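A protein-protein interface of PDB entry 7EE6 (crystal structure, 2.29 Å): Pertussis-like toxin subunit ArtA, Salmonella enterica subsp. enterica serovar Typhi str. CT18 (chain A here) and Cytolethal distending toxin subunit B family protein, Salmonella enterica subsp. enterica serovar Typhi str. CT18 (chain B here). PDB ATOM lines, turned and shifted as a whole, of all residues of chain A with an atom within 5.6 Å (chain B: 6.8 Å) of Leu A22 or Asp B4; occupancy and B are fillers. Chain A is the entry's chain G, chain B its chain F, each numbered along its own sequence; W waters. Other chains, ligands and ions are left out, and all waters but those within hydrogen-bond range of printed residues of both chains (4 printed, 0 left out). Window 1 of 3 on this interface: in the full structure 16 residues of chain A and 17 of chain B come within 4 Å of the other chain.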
ATOM      1  N   PHE A  20      21.668  12.139  -0.966  1.00  0.00           N
ATOM      2  CA  PHE A  20      23.073  12.290  -0.621  1.00  0.00           C
ATOM      3  C   PHE A  20      23.816  13.021  -1.735  1.00  0.00           C
ATOM      4  O   PHE A  20      23.639  12.714  -2.920  1.00  0.00           O
ATOM      5  CB  PHE A  20      23.732  10.934  -0.408  1.00  0.00           C
ATOM      6  CG  PHE A  20      23.199  10.161   0.746  1.00  0.00           C
ATOM      7  CD1 PHE A  20      23.408  10.597   2.048  1.00  0.00           C
ATOM      8  CD2 PHE A  20      22.544   8.954   0.543  1.00  0.00           C
ATOM      9  CE1 PHE A  20      22.951   9.859   3.136  1.00  0.00           C
ATOM     10  CE2 PHE A  20      22.070   8.200   1.633  1.00  0.00           C
ATOM     11  CZ  PHE A  20      22.275   8.658   2.930  1.00  0.00           C
ATOM     12  N   SER A  21      24.694  13.945  -1.358  1.00  0.00           N
ATOM     13  CA  SER A  21      25.331  14.819  -2.333  1.00  0.00           C
ATOM     14  C   SER A  21      26.845  14.574  -2.357  1.00  0.00           C
ATOM     15  O   SER A  21      27.443  14.173  -1.358  1.00  0.00           O
ATOM     16  CB  SER A  21      24.975  16.289  -2.013  1.00  0.00           C
ATOM     17  OG  SER A  21      25.451  17.164  -3.007  1.00  0.00           O
ATOM     18  N   LEU A  22      27.456  14.787  -3.521  1.00  0.00           N
ATOM     19  CA  LEU A  22      28.885  14.559  -3.700  1.00  0.00           C
ATOM     20  C   LEU A  22      29.712  15.615  -2.970  1.00  0.00           C
ATOM     21  O   LEU A  22      29.356  16.799  -2.921  1.00  0.00           O
ATOM     22  CB  LEU A  22      29.258  14.598  -5.181  1.00  0.00           C
ATOM     23  CG  LEU A  22      28.531  13.695  -6.161  1.00  0.00           C
ATOM     24  CD1 LEU A  22      29.017  14.022  -7.571  1.00  0.00           C
ATOM     25  CD2 LEU A  22      28.765  12.201  -5.827  1.00  0.00           C
ATOM     26  N   LEU A  23      30.857  15.188  -2.439  1.00  0.00           N
ATOM     27  CA  LEU A  23      31.742  16.154  -1.799  1.00  0.00           C
ATOM     28  C   LEU A  23      32.237  17.208  -2.794  1.00  0.00           C
ATOM     29  O   LEU A  23      32.258  18.408  -2.477  1.00  0.00           O
ATOM     30  CB  LEU A  23      32.915  15.426  -1.138  1.00  0.00           C
ATOM     31  CG  LEU A  23      32.665  14.870   0.269  1.00  0.00           C
ATOM     32  CD1 LEU A  23      33.967  14.387   0.876  1.00  0.00           C
ATOM     33  CD2 LEU A  23      32.004  15.893   1.159  1.00  0.00           C
ATOM     34  N   GLY A  24      32.605  16.791  -4.009  1.00  0.00           N
ATOM     35  CA  GLY A  24      33.231  17.702  -4.944  1.00  0.00           C
ATOM     36  C   GLY A  24      33.318  17.184  -6.368  1.00  0.00           C
ATOM     37  O   GLY A  24      32.456  16.429  -6.833  1.00  0.00           O
ATOM     38  N   TYR A  25      34.355  17.611  -7.085  1.00  0.00           N
ATOM     39  CA  TYR A  25      34.547  17.245  -8.481  1.00  0.00           C
ATOM     40  C   TYR A  25      35.733  16.299  -8.704  1.00  0.00           C
ATOM     41  O   TYR A  25      36.052  15.984  -9.857  1.00  0.00           O
ATOM     42  CB  TYR A  25      34.719  18.518  -9.318  1.00  0.00           C
ATOM     43  CG  TYR A  25      33.461  19.366  -9.450  1.00  0.00           C
ATOM     44  CD1 TYR A  25      32.336  18.865 -10.103  1.00  0.00           C
ATOM     45  CD2 TYR A  25      33.410  20.671  -8.962  1.00  0.00           C
ATOM     46  CE1 TYR A  25      31.191  19.615 -10.245  1.00  0.00           C
ATOM     47  CE2 TYR A  25      32.254  21.454  -9.108  1.00  0.00           C
ATOM     48  CZ  TYR A  25      31.147  20.911  -9.755  1.00  0.00           C
ATOM     49  OH  TYR A  25      29.987  21.637  -9.930  1.00  0.00           O
ATOM     50  N   SER A  45      35.731  14.498  -3.194  1.00  0.00           N
ATOM     51  CA  SER A  45      35.510  13.364  -4.069  1.00  0.00           C
ATOM     52  C   SER A  45      34.237  13.549  -4.878  1.00  0.00           C
ATOM     53  O   SER A  45      33.219  14.030  -4.369  1.00  0.00           O
ATOM     54  CB  SER A  45      35.418  12.093  -3.225  1.00  0.00           C
ATOM     55  OG  SER A  45      34.549  12.313  -2.115  1.00  0.00           O
ATOM     56  N   ARG A  46      34.304  13.164  -6.152  1.00  0.00           N
ATOM     57  CA  ARG A  46      33.148  13.121  -7.040  1.00  0.00           C
ATOM     58  C   ARG A  46      32.454  11.760  -7.015  1.00  0.00           C
ATOM     59  O   ARG A  46      31.906  11.319  -8.035  1.00  0.00           O
ATOM     60  CB  ARG A  46      33.579  13.482  -8.465  1.00  0.00           C
ATOM     61  CG  ARG A  46      32.493  14.120  -9.314  1.00  0.00           C
ATOM     62  CD  ARG A  46      33.078  14.607 -10.619  1.00  0.00           C
ATOM     63  NE  ARG A  46      32.094  15.278 -11.452  1.00  0.00           N
ATOM     64  CZ  ARG A  46      32.402  16.207 -12.358  1.00  0.00           C
ATOM     65  NH1 ARG A  46      33.666  16.581 -12.535  1.00  0.00           N
ATOM     66  NH2 ARG A  46      31.444  16.763 -13.074  1.00  0.00           N
ATOM     67  N   TYR A  47      32.485  11.073  -5.875  1.00  0.00           N
ATOM     68  CA  TYR A  47      31.899   9.749  -5.742  1.00  0.00           C
ATOM     69  C   TYR A  47      31.284   9.628  -4.361  1.00  0.00           C
ATOM     70  O   TYR A  47      31.715  10.290  -3.417  1.00  0.00           O
ATOM     71  CB  TYR A  47      32.936   8.613  -5.936  1.00  0.00           C
ATOM     72  CG  TYR A  47      33.774   8.708  -7.206  1.00  0.00           C
ATOM     73  CD1 TYR A  47      33.228   8.405  -8.447  1.00  0.00           C
ATOM     74  CD2 TYR A  47      35.107   9.070  -7.161  1.00  0.00           C
ATOM     75  CE1 TYR A  47      33.979   8.483  -9.612  1.00  0.00           C
ATOM     76  CE2 TYR A  47      35.871   9.139  -8.322  1.00  0.00           C
ATOM     77  CZ  TYR A  47      35.295   8.849  -9.538  1.00  0.00           C
ATOM     78  OH  TYR A  47      36.045   8.928 -10.697  1.00  0.00           O
ATOM     79  N   ILE A  48      30.254   8.791  -4.259  1.00  0.00           N
ATOM     80  CA  ILE A  48      29.686   8.390  -2.979  1.00  0.00           C
ATOM     81  C   ILE A  48      29.948   6.894  -2.830  1.00  0.00           C
ATOM     82  O   ILE A  48      29.567   6.104  -3.702  1.00  0.00           O
ATOM     83  CB  ILE A  48      28.179   8.705  -2.898  1.00  0.00           C
ATOM     84  CG1 ILE A  48      27.932  10.215  -2.894  1.00  0.00           C
ATOM     85  CG2 ILE A  48      27.581   8.100  -1.655  1.00  0.00           C
ATOM     86  CD1 ILE A  48      26.467  10.609  -2.964  1.00  0.00           C
ATOM     87  N   SER A 118      28.708   5.559  -6.422  1.00  0.00           N
ATOM     88  CA  SER A 118      27.820   6.378  -7.240  1.00  0.00           C
ATOM     89  C   SER A 118      28.611   7.543  -7.829  1.00  0.00           C
ATOM     90  O   SER A 118      29.248   8.294  -7.082  1.00  0.00           O
ATOM     91  CB  SER A 118      26.650   6.894  -6.405  1.00  0.00           C
ATOM     92  OG  SER A 118      25.659   7.476  -7.240  1.00  0.00           O
ATOM     93  N   THR A 119      28.562   7.691  -9.162  1.00  0.00           N
ATOM     94  CA  THR A 119      29.213   8.811  -9.842  1.00  0.00           C
ATOM     95  C   THR A 119      28.388  10.085  -9.804  1.00  0.00           C
ATOM     96  O   THR A 119      28.895  11.136 -10.215  1.00  0.00           O
ATOM     97  CB  THR A 119      29.509   8.488 -11.323  1.00  0.00           C
ATOM     98  OG1 THR A 119      28.292   8.129 -12.011  1.00  0.00           O
ATOM     99  CG2 THR A 119      30.522   7.359 -11.444  1.00  0.00           C
ATOM    100  N   LEU A 120      27.129   9.997  -9.363  1.00  0.00           N
ATOM    101  CA  LEU A 120      26.213  11.119  -9.199  1.00  0.00           C
ATOM    102  C   LEU A 120      25.699  11.151  -7.764  1.00  0.00           C
ATOM    103  O   LEU A 120      25.807  10.167  -7.011  1.00  0.00           O
ATOM    104  CB  LEU A 120      25.020  11.016 -10.163  1.00  0.00           C
ATOM    105  CG  LEU A 120      25.304  11.160 -11.660  1.00  0.00           C
ATOM    106  CD1 LEU A 120      24.010  10.972 -12.446  1.00  0.00           C
ATOM    107  CD2 LEU A 120      25.903  12.534 -11.944  1.00  0.00           C
ATOM    108  N   SER A 121      25.111  12.289  -7.394  1.00  0.00           N
ATOM    109  CA  SER A 121      24.358  12.344  -6.148  1.00  0.00           C
ATOM    110  C   SER A 121      23.288  11.254  -6.146  1.00  0.00           C
ATOM    111  O   SER A 121      22.802  10.824  -7.196  1.00  0.00           O
ATOM    112  CB  SER A 121      23.697  13.708  -5.980  1.00  0.00           C
ATOM    113  OG  SER A 121      24.659  14.711  -5.713  1.00  0.00           O
ATOM    114  N   VAL A 195      29.910  12.350   2.582  1.00  0.00           N
ATOM    115  CA  VAL A 195      28.911  12.885   1.668  1.00  0.00           C
ATOM    116  C   VAL A 195      28.605  14.294   2.145  1.00  0.00           C
ATOM    117  O   VAL A 195      28.776  14.601   3.331  1.00  0.00           O
ATOM    118  CB  VAL A 195      27.635  12.017   1.613  1.00  0.00           C
ATOM    119  CG1 VAL A 195      27.982  10.611   1.103  1.00  0.00           C
ATOM    120  CG2 VAL A 195      26.981  11.966   2.967  1.00  0.00           C
ATOM    121  N   CYS A 196      28.203  15.163   1.210  1.00  0.00           N
ATOM    122  CA  CYS A 196      27.886  16.546   1.541  1.00  0.00           C
ATOM    123  C   CYS A 196      26.518  16.640   2.198  1.00  0.00           C
ATOM    124  O   CYS A 196      25.534  16.089   1.690  1.00  0.00           O
ATOM    125  CB  CYS A 196      27.905  17.415   0.290  1.00  0.00           C
ATOM    126  SG  CYS A 196      27.892  19.172   0.684  1.00  0.00           S
ATOM    127  N   ASN B   1      22.269  15.358  -9.849  1.00  0.00           N
ATOM    128  CA  ASN B   1      21.928  16.678  -9.361  1.00  0.00           C
ATOM    129  C   ASN B   1      22.734  17.717 -10.133  1.00  0.00           C
ATOM    130  O   ASN B   1      23.780  17.388 -10.691  1.00  0.00           O
ATOM    131  CB  ASN B   1      22.196  16.777  -7.847  1.00  0.00           C
ATOM    132  CG  ASN B   1      21.200  15.968  -7.015  1.00  0.00           C
ATOM    133  OD1 ASN B   1      20.360  15.238  -7.550  1.00  0.00           O
ATOM    134  ND2 ASN B   1      21.291  16.098  -5.694  1.00  0.00           N
ATOM    135  N   ILE B   2      22.258  18.972 -10.158  1.00  0.00           N
ATOM    136  CA  ILE B   2      22.971  20.014 -10.897  1.00  0.00           C
ATOM    137  C   ILE B   2      24.394  20.160 -10.373  1.00  0.00           C
ATOM    138  O   ILE B   2      25.349  20.328 -11.144  1.00  0.00           O
ATOM    139  CB  ILE B   2      22.211  21.350 -10.816  1.00  0.00           C
ATOM    140  CG1 ILE B   2      20.728  21.137 -11.141  1.00  0.00           C
ATOM    141  CG2 ILE B   2      22.869  22.398 -11.727  1.00  0.00           C
ATOM    142  CD1 ILE B   2      20.463  20.659 -12.567  1.00  0.00           C
ATOM    143  N   SER B   3      24.555  20.095  -9.054  1.00  0.00           N
ATOM    144  CA  SER B   3      25.863  20.279  -8.449  1.00  0.00           C
ATOM    145  C   SER B   3      26.871  19.193  -8.854  1.00  0.00           C
ATOM    146  O   SER B   3      28.081  19.397  -8.682  1.00  0.00           O
ATOM    147  CB  SER B   3      25.685  20.363  -6.929  1.00  0.00           C
ATOM    148  OG  SER B   3      25.547  19.080  -6.360  1.00  0.00           O
ATOM    149  N   ASP B   4      26.416  18.058  -9.412  1.00  0.00           N
ATOM    150  CA  ASP B   4      27.347  17.024  -9.866  1.00  0.00           C
ATOM    151  C   ASP B   4      28.079  17.391 -11.150  1.00  0.00           C
ATOM    152  O   ASP B   4      29.028  16.687 -11.514  1.00  0.00           O
ATOM    153  CB  ASP B   4      26.634  15.695 -10.119  1.00  0.00           C
ATOM    154  CG  ASP B   4      25.813  15.212  -8.929  1.00  0.00           C
ATOM    155  OD1 ASP B   4      26.183  15.480  -7.755  1.00  0.00           O
ATOM    156  OD2 ASP B   4      24.772  14.571  -9.197  1.00  0.00           O
ATOM    157  N   TYR B   5      27.653  18.434 -11.863  1.00  0.00           N
ATOM    158  CA  TYR B   5      28.240  18.810 -13.146  1.00  0.00           C
ATOM    159  C   TYR B   5      28.940  20.162 -13.063  1.00  0.00           C
ATOM    160  O   TYR B   5      28.530  21.052 -12.310  1.00  0.00           O
ATOM    161  CB  TYR B   5      27.178  18.900 -14.245  1.00  0.00           C
ATOM    162  CG  TYR B   5      26.484  17.607 -14.528  1.00  0.00           C
ATOM    163  CD1 TYR B   5      25.444  17.163 -13.712  1.00  0.00           C
ATOM    164  CD2 TYR B   5      26.854  16.827 -15.624  1.00  0.00           C
ATOM    165  CE1 TYR B   5      24.784  15.967 -13.983  1.00  0.00           C
ATOM    166  CE2 TYR B   5      26.210  15.630 -15.898  1.00  0.00           C
ATOM    167  CZ  TYR B   5      25.183  15.204 -15.075  1.00  0.00           C
ATOM    168  OH  TYR B   5      24.554  14.010 -15.343  1.00  0.00           O
ATOM    169  N   LYS B   6      29.979  20.325 -13.867  1.00  0.00           N
ATOM    170  CA  LYS B   6      30.567  21.642 -14.098  1.00  0.00           C
ATOM    171  C   LYS B   6      29.814  22.257 -15.266  1.00  0.00           C
ATOM    172  O   LYS B   6      29.885  21.750 -16.392  1.00  0.00           O
ATOM    173  CB  LYS B   6      32.057  21.542 -14.400  1.00  0.00           C
ATOM    174  CG  LYS B   6      32.910  21.082 -13.233  1.00  0.00           C
ATOM    175  CD  LYS B   6      34.366  21.475 -13.481  1.00  0.00           C
ATOM    176  CE  LYS B   6      35.310  20.765 -12.523  1.00  0.00           C
ATOM    177  NZ  LYS B   6      36.704  21.263 -12.682  1.00  0.00           N
ATOM    178  N   VAL B   7      29.061  23.318 -14.992  1.00  0.00           N
ATOM    179  CA  VAL B   7      28.207  23.965 -15.986  1.00  0.00           C
ATOM    180  C   VAL B   7      28.808  25.333 -16.303  1.00  0.00           C
ATOM    181  O   VAL B   7      29.477  25.948 -15.462  1.00  0.00           O
ATOM    182  CB  VAL B   7      26.745  24.082 -15.476  1.00  0.00           C
ATOM    183  CG1 VAL B   7      25.793  24.513 -16.589  1.00  0.00           C
ATOM    184  CG2 VAL B   7      26.279  22.771 -14.816  1.00  0.00           C
ATOM    185  N   ASP B  38      31.531  20.244 -18.060  1.00  0.00           N
ATOM    186  CA  ASP B  38      30.703  19.117 -18.479  1.00  0.00           C
ATOM    187  C   ASP B  38      29.551  19.542 -19.362  1.00  0.00           C
ATOM    188  O   ASP B  38      29.198  18.835 -20.316  1.00  0.00           O
ATOM    189  CB  ASP B  38      30.155  18.388 -17.250  1.00  0.00           C
ATOM    190  CG  ASP B  38      31.257  17.900 -16.345  1.00  0.00           C
ATOM    191  OD1 ASP B  38      32.133  17.168 -16.864  1.00  0.00           O
ATOM    192  OD2 ASP B  38      31.275  18.272 -15.144  1.00  0.00           O
ATOM    193  N   ASP B 132      18.354  15.186 -14.577  1.00  0.00           N
ATOM    194  CA  ASP B 132      18.828  16.562 -14.672  1.00  0.00           C
ATOM    195  C   ASP B 132      18.607  17.086 -16.080  1.00  0.00           C
ATOM    196  O   ASP B 132      18.912  16.390 -17.061  1.00  0.00           O
ATOM    197  CB  ASP B 132      20.311  16.650 -14.290  1.00  0.00           C
ATOM    198  CG  ASP B 132      20.544  16.261 -12.841  1.00  0.00           C
ATOM    199  OD1 ASP B 132      19.741  16.701 -11.986  1.00  0.00           O
ATOM    200  OD2 ASP B 132      21.507  15.499 -12.552  1.00  0.00           O
ATOM    201  N   TYR B 221      19.948  20.062  -3.359  1.00  0.00           N
ATOM    202  CA  TYR B 221      21.229  20.751  -3.213  1.00  0.00           C
ATOM    203  C   TYR B 221      21.404  21.859  -4.254  1.00  0.00           C
ATOM    204  O   TYR B 221      22.532  22.200  -4.632  1.00  0.00           O
ATOM    205  CB  TYR B 221      22.405  19.756  -3.236  1.00  0.00           C
ATOM    206  CG  TYR B 221      22.344  18.770  -2.081  1.00  0.00           C
ATOM    207  CD1 TYR B 221      22.856  19.093  -0.825  1.00  0.00           C
ATOM    208  CD2 TYR B 221      21.722  17.536  -2.235  1.00  0.00           C
ATOM    209  CE1 TYR B 221      22.763  18.201   0.241  1.00  0.00           C
ATOM    210  CE2 TYR B 221      21.629  16.642  -1.179  1.00  0.00           C
ATOM    211  CZ  TYR B 221      22.155  16.977   0.055  1.00  0.00           C
ATOM    212  OH  TYR B 221      22.056  16.067   1.085  1.00  0.00           O
ATOM    213  N   ARG B 224      23.836  24.728  -3.496  1.00  0.00           N
ATOM    214  CA  ARG B 224      25.284  24.598  -3.587  1.00  0.00           C
ATOM    215  C   ARG B 224      25.840  25.239  -4.844  1.00  0.00           C
ATOM    216  O   ARG B 224      27.049  25.483  -4.913  1.00  0.00           O
ATOM    217  CB  ARG B 224      25.698  23.129  -3.571  1.00  0.00           C
ATOM    218  CG  ARG B 224      25.473  22.409  -2.257  1.00  0.00           C
ATOM    219  CD  ARG B 224      26.093  21.038  -2.299  1.00  0.00           C
ATOM    220  NE  ARG B 224      27.550  21.100  -2.344  1.00  0.00           N
ATOM    221  CZ  ARG B 224      28.333  20.101  -2.747  1.00  0.00           C
ATOM    222  NH1 ARG B 224      27.802  18.946  -3.153  1.00  0.00           N
ATOM    223  NH2 ARG B 224      29.653  20.252  -2.741  1.00  0.00           N
ATOM    224  N   VAL B 225      25.003  25.486  -5.844  1.00  0.00           N
ATOM    225  CA  VAL B 225      25.498  25.941  -7.139  1.00  0.00           C
ATOM    226  C   VAL B 225      25.756  27.441  -7.070  1.00  0.00           C
ATOM    227  O   VAL B 225      24.866  28.227  -6.717  1.00  0.00           O
ATOM    228  CB  VAL B 225      24.521  25.586  -8.266  1.00  0.00           C
ATOM    229  CG1 VAL B 225      25.105  26.003  -9.610  1.00  0.00           C
ATOM    230  CG2 VAL B 225      24.230  24.090  -8.257  1.00  0.00           C
ATOM    231  N   ALA B 244      29.574  23.708  -7.860  1.00  0.00           N
ATOM    232  CA  ALA B 244      29.208  23.388  -6.497  1.00  0.00           C
ATOM    233  C   ALA B 244      30.230  23.982  -5.543  1.00  0.00           C
ATOM    234  O   ALA B 244      31.436  23.891  -5.775  1.00  0.00           O
ATOM    235  CB  ALA B 244      29.117  21.875  -6.325  1.00  0.00           C
ATOM    236  N   ARG B 245      29.741  24.616  -4.483  1.00  0.00           N
ATOM    237  CA  ARG B 245      30.609  25.118  -3.436  1.00  0.00           C
ATOM    238  C   ARG B 245      31.243  23.957  -2.684  1.00  0.00           C
ATOM    239  O   ARG B 245      30.700  22.840  -2.623  1.00  0.00           O
ATOM    240  CB  ARG B 245      29.831  25.990  -2.448  1.00  0.00           C
ATOM    241  CG  ARG B 245      29.222  27.224  -3.054  1.00  0.00           C
ATOM    242  CD  ARG B 245      28.364  27.978  -2.032  1.00  0.00           C
ATOM    243  NE  ARG B 245      28.121  29.369  -2.431  1.00  0.00           N
ATOM    244  CZ  ARG B 245      27.010  29.799  -3.026  1.00  0.00           C
ATOM    245  NH1 ARG B 245      26.024  28.947  -3.288  1.00  0.00           N
ATOM    246  NH2 ARG B 245      26.877  31.085  -3.349  1.00  0.00           N
ATOM    247  N   CYS B 247      31.984  21.637   0.261  1.00  0.00           N
ATOM    248  CA  CYS B 247      31.026  21.252   1.284  1.00  0.00           C
ATOM    249  C   CYS B 247      31.466  21.768   2.652  1.00  0.00           C
ATOM    250  O   CYS B 247      30.721  22.497   3.318  1.00  0.00           O
ATOM    251  CB  CYS B 247      30.834  19.740   1.273  1.00  0.00           C
ATOM    252  SG  CYS B 247      29.347  19.335   2.112  1.00  0.00           S
HETATM  253  O   HOH W   1      26.946  22.992 -10.790  1.00  0.00           O
HETATM  254  O   HOH W   2      23.936  17.218  -5.019  1.00  0.00           O
HETATM  255  O   HOH W   3      21.390  12.701  -9.148  1.00  0.00           O
HETATM  256  O   HOH W   4      29.848  17.905  -6.901  1.00  0.00           O
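Of chain B, only Asp B4 (3.2 Å) and Arg B224 (2.7 Å) come within 4 Å of Leu A22. Asp B4 touches five residues of chain A. Printed residues of chain A within 4 Å of Lys B6: Tyr A25 (3.7 Å) and Arg A46 (3.9 Å). Of the printed residues of chain B, Tyr A25 touches Ser B3 (3.2 Å), Asp B4 (3.9 Å), Tyr B5 (2.9 Å), Lys B6 (3.7 Å) and Ala B244 (3.0 Å). Of the printed residues of chain A, Asn B1 touches Ser A121. The nearest residue of chain B that does not touch Leu A22 is Cys B247 (5.3 Å). The nearest printed residue of chain A that does not touch Asp B4 is Thr A119 (5.1 Å). The nearest printed residue of chain B that does not touch Leu A23 is Cys B247 (4.02 Å).
Of the 16 printed residues of chain A, 8 touch a printed residue of chain B. Printed residues of chain A that touch a printed residue of chain B: Ser A21, Leu A22, Leu A23, Tyr A25, Arg A46, Leu A120, Ser A121 and Cys A196. Of the 15 printed residues of chain B, 10 touch a printed residue of chain A. Hydrophobic or aromatic side chains of chain B within 4 Å of the printed part of chain A: Tyr B5, Tyr B221 and Ala B244. Among the printed residues, 22 pairs touch across the chains.
OG of Ser A21 touches OG of Ser B3, at 3.9 Å. Tyr B221 touches Ser A21. Leu A22 touches Asp B4. O of Asp B4 touches CE1 of Tyr A25 (3.9 Å). CG of Lys B6 touches CE1 of Tyr A25, 3.7 Å away. NH2 of Arg A46 touches CA of Tyr B5 (3.8 Å). NH2 of Arg A46 touches N of Lys B6 (3.9 Å). CD2 of Leu A120 touches OD2 of Asp B4 (3.6 Å). Ser A121 touches Asn B1 (CB to ND2, 3.4 Å). OH of Tyr B221 touches O of Cys A196, at 3.5 Å.
The side-chain hydroxyl (OH) of Tyr A25 lies within hydrogen-bond range of the backbone carbonyl oxygen (O) of Ser B3 (3.2 Å). O of Asp B4 sits at hydrogen-bond distance from NH2 of Arg A46 (2.9 Å). OG of Ser A121 lies within hydrogen-bond range of OD1 of Asp B4 (2.7 Å). OH of Tyr A25 sits at hydrogen-bond distance from O of Tyr B5, at 2.9 Å. The side-chain carboxylate (OD2) of Asp B38 lies within salt-bridge range of the guanidinium group (NH2) of Arg A46 (2.6 Å). The guanidinium group of Arg B224 lies within hydrogen-bond range of the side-chain hydroxyl of Ser A21, 3.0 Å away. NH1 of Arg B224 is in hydrogen-bond range of O of Leu A22, at 2.7 Å. NH2 of Arg B224 is in hydrogen-bond range of O of Leu A23 (3.2 Å). The guanidinium group (NE) of Arg B224 lies close to the side-chain sulfur (SG) of Cys A196 (3.6 Å). OH of Tyr A25 lies within hydrogen-bond range of N of Ala B244 (3.0 Å). SG of Cys A196 is disulfide-bonded to SG of Cys B247 (2.0 Å).
Water W2 lies within hydrogen-bond range of the side-chain hydroxyl (OG) of Ser A21, the side-chain hydroxyl (OG) of Ser A121, the side-chain hydroxyl (OG) of Ser B3 and the side-chain amide nitrogen (ND2) of Asn B1. Water W3 lies within hydrogen-bond range of N of Asn B1 (2.9 Å) and O of Ser A121 (3.1 Å). Water W4 lies within hydrogen-bond range of O of Ser B3 and O of Gly A24. Water W1 lies within hydrogen-bond range of the backbone carbonyl oxygen (O) of Tyr B5 (2.9 Å), the backbone carbonyl oxygen (O) of Ile B2 (3.1 Å) and the side-chain hydroxyl (OH) of Tyr A25 (3.4 Å).
The backbone NH of Asn B1 lies within hydrogen-bond range of the side-chain carboxylate of Asp B132, at 2.8 Å. The side-chain carboxylate (OD2) of Asp B38 sits at hydrogen-bond distance from the backbone NH (N) of Lys B6. The backbone carbonyl oxygen (O) of Arg B245 lies within hydrogen-bond range of the guanidinium group (NH2) of Arg B224 (2.8 Å). The backbone NH (N) of Cys A196 lies within hydrogen-bond range of the backbone carbonyl oxygen (O) of Ser A21. The backbone carbonyl oxygen (O) of Ser A45 sits at hydrogen-bond distance from the backbone NH (N) of Leu A23 (3.3 Å). O of Leu A120 lies within hydrogen-bond range of OG of Ser A118, 2.7 Å away.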
